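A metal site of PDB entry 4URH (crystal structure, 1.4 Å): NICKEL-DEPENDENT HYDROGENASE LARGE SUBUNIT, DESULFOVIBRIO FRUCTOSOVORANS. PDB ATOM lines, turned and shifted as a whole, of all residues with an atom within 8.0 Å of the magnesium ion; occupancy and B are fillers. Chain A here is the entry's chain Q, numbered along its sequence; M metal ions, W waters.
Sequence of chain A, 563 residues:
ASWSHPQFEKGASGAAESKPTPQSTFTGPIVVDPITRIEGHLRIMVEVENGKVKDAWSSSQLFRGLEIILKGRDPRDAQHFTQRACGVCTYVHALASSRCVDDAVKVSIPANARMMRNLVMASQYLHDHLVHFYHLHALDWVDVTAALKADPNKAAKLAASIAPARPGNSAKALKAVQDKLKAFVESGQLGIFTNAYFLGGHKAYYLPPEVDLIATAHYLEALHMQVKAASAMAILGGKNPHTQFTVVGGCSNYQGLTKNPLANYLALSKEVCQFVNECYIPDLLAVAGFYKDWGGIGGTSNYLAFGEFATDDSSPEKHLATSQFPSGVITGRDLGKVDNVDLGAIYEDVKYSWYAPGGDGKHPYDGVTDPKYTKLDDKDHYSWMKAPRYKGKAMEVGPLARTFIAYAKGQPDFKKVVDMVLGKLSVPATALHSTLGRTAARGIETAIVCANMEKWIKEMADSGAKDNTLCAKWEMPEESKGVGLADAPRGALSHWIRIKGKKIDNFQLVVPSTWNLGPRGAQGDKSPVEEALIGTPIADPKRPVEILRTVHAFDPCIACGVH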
ATOM      1  N   PHE A  63      -9.102   9.296  17.254  1.00  0.00           N
ATOM      2  CA  PHE A  63      -8.660   8.025  16.711  1.00  0.00           C
ATOM      3  C   PHE A  63      -8.109   8.273  15.297  1.00  0.00           C
ATOM      4  O   PHE A  63      -8.742   8.993  14.506  1.00  0.00           O
ATOM      5  CB  PHE A  63      -9.883   7.058  16.595  1.00  0.00           C
ATOM      6  CG  PHE A  63      -9.511   5.713  16.020  1.00  0.00           C
ATOM      7  CD1 PHE A  63      -8.887   4.739  16.824  1.00  0.00           C
ATOM      8  CD2 PHE A  63      -9.771   5.401  14.683  1.00  0.00           C
ATOM      9  CE1 PHE A  63      -8.515   3.493  16.337  1.00  0.00           C
ATOM     10  CE2 PHE A  63      -9.401   4.144  14.166  1.00  0.00           C
ATOM     11  CZ  PHE A  63      -8.801   3.196  14.999  1.00  0.00           C
ATOM     12  N   GLU A  67      -2.922   0.976  13.008  1.00  0.00           N
ATOM     13  CA  GLU A  67      -2.856  -0.479  12.941  1.00  0.00           C
ATOM     14  C   GLU A  67      -3.720  -0.994  11.782  1.00  0.00           C
ATOM     15  O   GLU A  67      -3.346  -1.960  11.132  1.00  0.00           O
ATOM     16  CB  GLU A  67      -3.333  -1.105  14.239  1.00  0.00           C
ATOM     17  CG  GLU A  67      -2.386  -0.816  15.428  1.00  0.00           C
ATOM     18  CD  GLU A  67      -3.088  -0.857  16.761  1.00  0.00           C
ATOM     19  OE1 GLU A  67      -4.344  -0.735  16.817  1.00  0.00           O
ATOM     20  OE2 GLU A  67      -2.404  -1.021  17.798  1.00  0.00           O
ATOM     21  N   GLU A 348      -4.832  -6.555  26.057  1.00  0.00           N
ATOM     22  CA  GLU A 348      -5.579  -5.285  26.067  1.00  0.00           C
ATOM     23  C   GLU A 348      -7.077  -5.555  26.100  1.00  0.00           C
ATOM     24  O   GLU A 348      -7.585  -6.438  25.364  1.00  0.00           O
ATOM     25  CB  GLU A 348      -5.288  -4.444  24.835  1.00  0.00           C
ATOM     26  CG  GLU A 348      -3.824  -3.977  24.809  1.00  0.00           C
ATOM     27  CD  GLU A 348      -3.509  -3.200  23.552  1.00  0.00           C
ATOM     28  OE1 GLU A 348      -3.457  -3.799  22.442  1.00  0.00           O
ATOM     29  OE2 GLU A 348      -3.304  -1.947  23.673  1.00  0.00           O
ATOM     30  N   TYR A 355     -14.534   0.577  20.926  1.00  0.00           N
ATOM     31  CA  TYR A 355     -14.286  -0.550  20.017  1.00  0.00           C
ATOM     32  C   TYR A 355     -15.455  -1.515  20.106  1.00  0.00           C
ATOM     33  O   TYR A 355     -16.239  -1.446  21.052  1.00  0.00           O
ATOM     34  CB  TYR A 355     -12.934  -1.236  20.242  1.00  0.00           C
ATOM     35  CG  TYR A 355     -11.769  -0.260  20.052  1.00  0.00           C
ATOM     36  CD1 TYR A 355     -11.241  -0.014  18.781  1.00  0.00           C
ATOM     37  CD2 TYR A 355     -11.309   0.449  21.122  1.00  0.00           C
ATOM     38  CE1 TYR A 355     -10.227   0.938  18.596  1.00  0.00           C
ATOM     39  CE2 TYR A 355     -10.286   1.391  20.971  1.00  0.00           C
ATOM     40  CZ  TYR A 355      -9.754   1.630  19.706  1.00  0.00           C
ATOM     41  OH  TYR A 355      -8.775   2.575  19.499  1.00  0.00           O
ATOM     42  N   PRO A 364      -1.385  -8.931  22.222  1.00  0.00           N
ATOM     43  CA  PRO A 364      -1.242  -8.116  21.009  1.00  0.00           C
ATOM     44  C   PRO A 364      -0.907  -8.881  19.704  1.00  0.00           C
ATOM     45  O   PRO A 364      -1.211  -8.369  18.625  1.00  0.00           O
ATOM     46  CB  PRO A 364      -0.087  -7.177  21.365  1.00  0.00           C
ATOM     47  CG  PRO A 364      -0.058  -7.124  22.868  1.00  0.00           C
ATOM     48  CD  PRO A 364      -0.458  -8.501  23.309  1.00  0.00           C
ATOM     49  N   GLY A 367      -4.200  -9.092  18.480  1.00  0.00           N
ATOM     50  CA  GLY A 367      -4.920  -7.860  18.714  1.00  0.00           C
ATOM     51  C   GLY A 367      -5.956  -7.551  17.617  1.00  0.00           C
ATOM     52  O   GLY A 367      -5.810  -7.957  16.455  1.00  0.00           O
ATOM     53  N   VAL A 368      -7.006  -6.823  18.009  1.00  0.00           N
ATOM     54  CA  VAL A 368      -8.117  -6.423  17.132  1.00  0.00           C
ATOM     55  C   VAL A 368      -8.376  -4.952  17.311  1.00  0.00           C
ATOM     56  O   VAL A 368      -8.435  -4.461  18.444  1.00  0.00           O
ATOM     57  CB  VAL A 368      -9.411  -7.203  17.533  1.00  0.00           C
ATOM     58  CG1 VAL A 368     -10.584  -6.836  16.618  1.00  0.00           C
ATOM     59  CG2 VAL A 368      -9.147  -8.703  17.533  1.00  0.00           C
ATOM     60  N   THR A 369      -8.506  -4.215  16.207  1.00  0.00           N
ATOM     61  CA  THR A 369      -8.777  -2.778  16.284  1.00  0.00           C
ATOM     62  C   THR A 369      -9.990  -2.458  15.419  1.00  0.00           C
ATOM     63  O   THR A 369      -9.882  -2.213  14.217  1.00  0.00           O
ATOM     64  CB  THR A 369      -7.512  -1.982  15.869  1.00  0.00           C
ATOM     65  OG1 THR A 369      -6.400  -2.470  16.637  1.00  0.00           O
ATOM     66  CG2 THR A 369      -7.703  -0.480  16.063  1.00  0.00           C
ATOM     67  N   TRP A 384     -10.896   6.423  23.171  1.00  0.00           N
ATOM     68  CA  TRP A 384     -10.292   5.766  22.030  1.00  0.00           C
ATOM     69  C   TRP A 384      -9.043   4.916  22.398  1.00  0.00           C
ATOM     70  O   TRP A 384      -8.552   4.144  21.567  1.00  0.00           O
ATOM     71  CB  TRP A 384      -9.924   6.797  20.968  1.00  0.00           C
ATOM     72  CG  TRP A 384     -11.088   7.304  20.235  1.00  0.00           C
ATOM     73  CD1 TRP A 384     -11.635   8.546  20.298  1.00  0.00           C
ATOM     74  CD2 TRP A 384     -11.919   6.536  19.335  1.00  0.00           C
ATOM     75  NE1 TRP A 384     -12.749   8.629  19.473  1.00  0.00           N
ATOM     76  CE2 TRP A 384     -12.944   7.420  18.866  1.00  0.00           C
ATOM     77  CE3 TRP A 384     -11.865   5.232  18.823  1.00  0.00           C
ATOM     78  CZ2 TRP A 384     -13.915   7.008  17.892  1.00  0.00           C
ATOM     79  CZ3 TRP A 384     -12.855   4.815  17.904  1.00  0.00           C
ATOM     80  CH2 TRP A 384     -13.855   5.728  17.439  1.00  0.00           C
ATOM     81  N   MET A 385      -8.535   5.032  23.642  1.00  0.00           N
ATOM     82  CA  MET A 385      -7.464   4.106  24.017  1.00  0.00           C
ATOM     83  C   MET A 385      -8.043   2.761  24.466  1.00  0.00           C
ATOM     84  O   MET A 385      -9.113   2.714  25.113  1.00  0.00           O
ATOM     85  CB  MET A 385      -6.651   4.645  25.168  1.00  0.00           C
ATOM     86  CG  MET A 385      -5.788   5.875  24.805  1.00  0.00           C
ATOM     87  SD  MET A 385      -4.574   6.120  26.139  1.00  0.00           S
ATOM     88  CE  MET A 385      -3.986   7.799  25.792  1.00  0.00           C
ATOM     89  N   LYS A 386      -7.340   1.687  24.116  1.00  0.00           N
ATOM     90  CA  LYS A 386      -7.558   0.388  24.768  1.00  0.00           C
ATOM     91  C   LYS A 386      -7.045   0.444  26.202  1.00  0.00           C
ATOM     92  O   LYS A 386      -6.359   1.417  26.597  1.00  0.00           O
ATOM     93  CB  LYS A 386      -6.889  -0.742  23.985  1.00  0.00           C
ATOM     94  CG  LYS A 386      -7.318  -0.792  22.510  1.00  0.00           C
ATOM     95  CD  LYS A 386      -6.685  -1.988  21.768  1.00  0.00           C
ATOM     96  CE  LYS A 386      -7.169  -2.092  20.309  1.00  0.00           C
ATOM     97  NZ  LYS A 386      -6.225  -2.990  19.537  1.00  0.00           N
ATOM     98  N   PRO A 388      -4.563  -1.598  28.440  1.00  0.00           N
ATOM     99  CA  PRO A 388      -3.621  -2.703  28.571  1.00  0.00           C
ATOM    100  C   PRO A 388      -3.549  -3.169  30.021  1.00  0.00           C
ATOM    101  O   PRO A 388      -3.601  -2.345  30.935  1.00  0.00           O
ATOM    102  CB  PRO A 388      -2.270  -2.054  28.162  1.00  0.00           C
ATOM    103  CG  PRO A 388      -2.664  -0.793  27.426  1.00  0.00           C
ATOM    104  CD  PRO A 388      -3.878  -0.326  28.194  1.00  0.00           C
ATOM    105  N   SER A 494       5.797  -1.400  23.043  1.00  0.00           N
ATOM    106  CA  SER A 494       5.960  -2.660  22.305  1.00  0.00           C
ATOM    107  C   SER A 494       5.150  -2.625  20.997  1.00  0.00           C
ATOM    108  O   SER A 494       3.985  -2.138  20.977  1.00  0.00           O
ATOM    109  CB  SER A 494       5.598  -3.879  23.185  1.00  0.00           C
ATOM    110  OG  SER A 494       4.283  -3.765  23.748  1.00  0.00           O
ATOM    111  N   TRP A 496       4.113  -5.255  17.765  1.00  0.00           N
ATOM    112  CA  TRP A 496       3.954  -6.710  17.590  1.00  0.00           C
ATOM    113  C   TRP A 496       3.456  -6.993  16.173  1.00  0.00           C
ATOM    114  O   TRP A 496       2.406  -6.448  15.773  1.00  0.00           O
ATOM    115  CB  TRP A 496       2.879  -7.223  18.578  1.00  0.00           C
ATOM    116  CG  TRP A 496       3.095  -6.809  19.998  1.00  0.00           C
ATOM    117  CD1 TRP A 496       2.836  -5.554  20.532  1.00  0.00           C
ATOM    118  CD2 TRP A 496       3.512  -7.631  21.087  1.00  0.00           C
ATOM    119  NE1 TRP A 496       3.124  -5.553  21.877  1.00  0.00           N
ATOM    120  CE2 TRP A 496       3.545  -6.810  22.251  1.00  0.00           C
ATOM    121  CE3 TRP A 496       3.901  -8.966  21.200  1.00  0.00           C
ATOM    122  CZ2 TRP A 496       3.931  -7.288  23.510  1.00  0.00           C
ATOM    123  CZ3 TRP A 496       4.306  -9.457  22.432  1.00  0.00           C
ATOM    124  CH2 TRP A 496       4.323  -8.625  23.586  1.00  0.00           C
ATOM    125  N   PHE A 507      -0.562  -5.836  12.857  1.00  0.00           N
ATOM    126  CA  PHE A 507       0.498  -5.019  13.452  1.00  0.00           C
ATOM    127  C   PHE A 507      -0.185  -4.254  14.569  1.00  0.00           C
ATOM    128  O   PHE A 507      -1.109  -3.483  14.322  1.00  0.00           O
ATOM    129  CB  PHE A 507       1.134  -4.041  12.426  1.00  0.00           C
ATOM    130  CG  PHE A 507       2.487  -3.553  12.857  1.00  0.00           C
ATOM    131  CD1 PHE A 507       2.574  -2.625  13.870  1.00  0.00           C
ATOM    132  CD2 PHE A 507       3.664  -4.047  12.277  1.00  0.00           C
ATOM    133  CE1 PHE A 507       3.847  -2.176  14.317  1.00  0.00           C
ATOM    134  CE2 PHE A 507       4.896  -3.614  12.711  1.00  0.00           C
ATOM    135  CZ  PHE A 507       4.986  -2.693  13.730  1.00  0.00           C
ATOM    136  N   GLN A 508       0.267  -4.504  15.799  1.00  0.00           N
ATOM    137  CA  GLN A 508      -0.355  -3.889  16.949  1.00  0.00           C
ATOM    138  C   GLN A 508       0.681  -3.085  17.760  1.00  0.00           C
ATOM    139  O   GLN A 508       1.771  -3.591  18.052  1.00  0.00           O
ATOM    140  CB  GLN A 508      -1.000  -4.976  17.832  1.00  0.00           C
ATOM    141  CG  GLN A 508      -2.190  -5.686  17.172  1.00  0.00           C
ATOM    142  CD  GLN A 508      -3.414  -4.810  17.105  1.00  0.00           C
ATOM    143  OE1 GLN A 508      -3.713  -4.093  18.063  1.00  0.00           O
ATOM    144  NE2 GLN A 508      -4.148  -4.862  15.985  1.00  0.00           N
ATOM    145  N   LEU A 509       0.306  -1.871  18.145  1.00  0.00           N
ATOM    146  CA  LEU A 509       1.187  -1.065  19.029  1.00  0.00           C
ATOM    147  C   LEU A 509       0.540  -1.052  20.397  1.00  0.00           C
ATOM    148  O   LEU A 509      -0.701  -0.879  20.489  1.00  0.00           O
ATOM    149  CB  LEU A 509       1.237   0.396  18.552  1.00  0.00           C
ATOM    150  CG  LEU A 509       1.851   0.720  17.194  1.00  0.00           C
ATOM    151  CD1 LEU A 509       0.974   0.351  16.019  1.00  0.00           C
ATOM    152  CD2 LEU A 509       2.075   2.223  17.189  1.00  0.00           C
ATOM    153  N   VAL A 510       1.335  -1.213  21.459  1.00  0.00           N
ATOM    154  CA  VAL A 510       0.861  -1.054  22.840  1.00  0.00           C
ATOM    155  C   VAL A 510       1.850  -0.058  23.443  1.00  0.00           C
ATOM    156  O   VAL A 510       3.064  -0.347  23.510  1.00  0.00           O
ATOM    157  CB  VAL A 510       0.846  -2.369  23.625  1.00  0.00           C
ATOM    158  CG1 VAL A 510       0.213  -2.152  25.033  1.00  0.00           C
ATOM    159  CG2 VAL A 510       0.071  -3.463  22.848  1.00  0.00           C
ATOM    160  N   VAL A 511       1.359   1.125  23.787  1.00  0.00           N
ATOM    161  CA  VAL A 511       2.254   2.296  23.936  1.00  0.00           C
ATOM    162  C   VAL A 511       2.218   2.765  25.397  1.00  0.00           C
ATOM    163  O   VAL A 511       1.224   2.520  26.130  1.00  0.00           O
ATOM    164  CB  VAL A 511       1.798   3.379  22.918  1.00  0.00           C
ATOM    165  CG1 VAL A 511       2.748   4.570  22.860  1.00  0.00           C
ATOM    166  CG2 VAL A 511       1.699   2.757  21.515  1.00  0.00           C
ATOM    167  N   THR A 514      -0.830   4.396  26.561  1.00  0.00           N
ATOM    168  CA  THR A 514      -1.967   3.431  26.599  1.00  0.00           C
ATOM    169  C   THR A 514      -1.998   2.805  27.996  1.00  0.00           C
ATOM    170  O   THR A 514      -3.049   2.763  28.640  1.00  0.00           O
ATOM    171  CB  THR A 514      -1.844   2.328  25.539  1.00  0.00           C
ATOM    172  OG1 THR A 514      -1.310   2.849  24.315  1.00  0.00           O
ATOM    173  CG2 THR A 514      -3.298   1.823  25.210  1.00  0.00           C
ATOM    174  N   CYS A 560       0.215   8.958  20.712  1.00  0.00           N
ATOM    175  CA  CYS A 560       0.858   7.681  21.053  1.00  0.00           C
ATOM    176  C   CYS A 560      -0.166   6.683  21.573  1.00  0.00           C
ATOM    177  O   CYS A 560      -0.167   5.529  21.157  1.00  0.00           O
ATOM    178  CB  CYS A 560       1.921   7.865  22.150  1.00  0.00           C
ATOM    179  SG  CYS A 560       3.561   8.131  21.530  1.00  0.00           S
ATOM    180  N   GLY A 561      -0.945   7.118  22.543  1.00  0.00           N
ATOM    181  CA  GLY A 561      -1.797   6.171  23.294  1.00  0.00           C
ATOM    182  C   GLY A 561      -2.874   5.492  22.458  1.00  0.00           C
ATOM    183  O   GLY A 561      -3.135   4.306  22.668  1.00  0.00           O
ATOM    184  N   VAL A 562      -3.431   6.213  21.474  1.00  0.00           N
ATOM    185  CA  VAL A 562      -4.515   5.678  20.649  1.00  0.00           C
ATOM    186  C   VAL A 562      -3.994   5.164  19.312  1.00  0.00           C
ATOM    187  O   VAL A 562      -4.428   4.123  18.809  1.00  0.00           O
ATOM    188  CB  VAL A 562      -5.559   6.767  20.322  1.00  0.00           C
ATOM    189  CG1 VAL A 562      -6.645   6.176  19.414  1.00  0.00           C
ATOM    190  CG2 VAL A 562      -6.170   7.331  21.604  1.00  0.00           C
ATOM    191  N   HIS A 563      -3.042   5.905  18.704  1.00  0.00           N
ATOM    192  CA  HIS A 563      -2.536   5.587  17.362  1.00  0.00           C
ATOM    193  C   HIS A 563      -3.696   5.267  16.374  1.00  0.00           C
ATOM    194  O   HIS A 563      -3.617   4.307  15.596  1.00  0.00           O
ATOM    195  CB  HIS A 563      -1.386   4.510  17.410  1.00  0.00           C
ATOM    196  CG  HIS A 563      -1.634   3.386  18.357  1.00  0.00           C
ATOM    197  ND1 HIS A 563      -1.384   3.493  19.719  1.00  0.00           N
ATOM    198  CD2 HIS A 563      -2.144   2.137  18.163  1.00  0.00           C
ATOM    199  CE1 HIS A 563      -1.747   2.361  20.321  1.00  0.00           C
ATOM    200  NE2 HIS A 563      -2.213   1.528  19.403  1.00  0.00           N
ATOM    201  OXT HIS A 563      -4.691   6.006  16.346  1.00  0.00           O
HETATM  202 MG    MG M   1      -2.758  -0.552  19.858  1.00  0.00          MG
HETATM  203  O   HOH W   1      -4.779  -0.253  19.406  1.00  0.00           O
HETATM  204  O   HOH W   2      -3.196  -0.035  21.838  1.00  0.00           O
HETATM  205  O   HOH W   3      -3.133  -2.530  20.207  1.00  0.00           O
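OE1 of Glu 67 lies within hydrogen-bond range of OG1 of Thr 369 (2.7 Å).
OE2 of Glu 67 lies close to OE1 of Gln 508 (3.3 Å).
A ring nitrogen (ND1) of His 563 lies within hydrogen-bond range of the backbone carbonyl oxygen of Cys 560, 2.8 Å away.
Of the 24 residues printed, 3 come within 4 Å of the magnesium ion.
The nearest printed residue that does not touch the magnesium ion is Gln 508 (4.1 Å).
Water W3 lies within hydrogen-bond range of the side-chain carboxylate (OE1) of Glu 348 (2.6 Å), the side-chain amide oxygen (OE1) of Gln 508 (2.7 Å) and the side-chain amino group (NZ) of Lys 386 (3.2 Å).
Water W1 bridges the side-chain carboxylate (OE1) of Glu 67 and the side-chain amino group (NZ) of Lys 386.
The magnesium ion is bound by water W3 (2.0 Å), water W1 (2.1 Å), water W2 (2.1 Å), the side-chain carboxylate of Glu 67 (2.1 Å), the backbone carbonyl oxygen of Leu 509 (2.2 Å) and a ring nitrogen (NE2) of His 563 (2.2 Å).
The magnesium ion has six donor atoms within binding distance.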
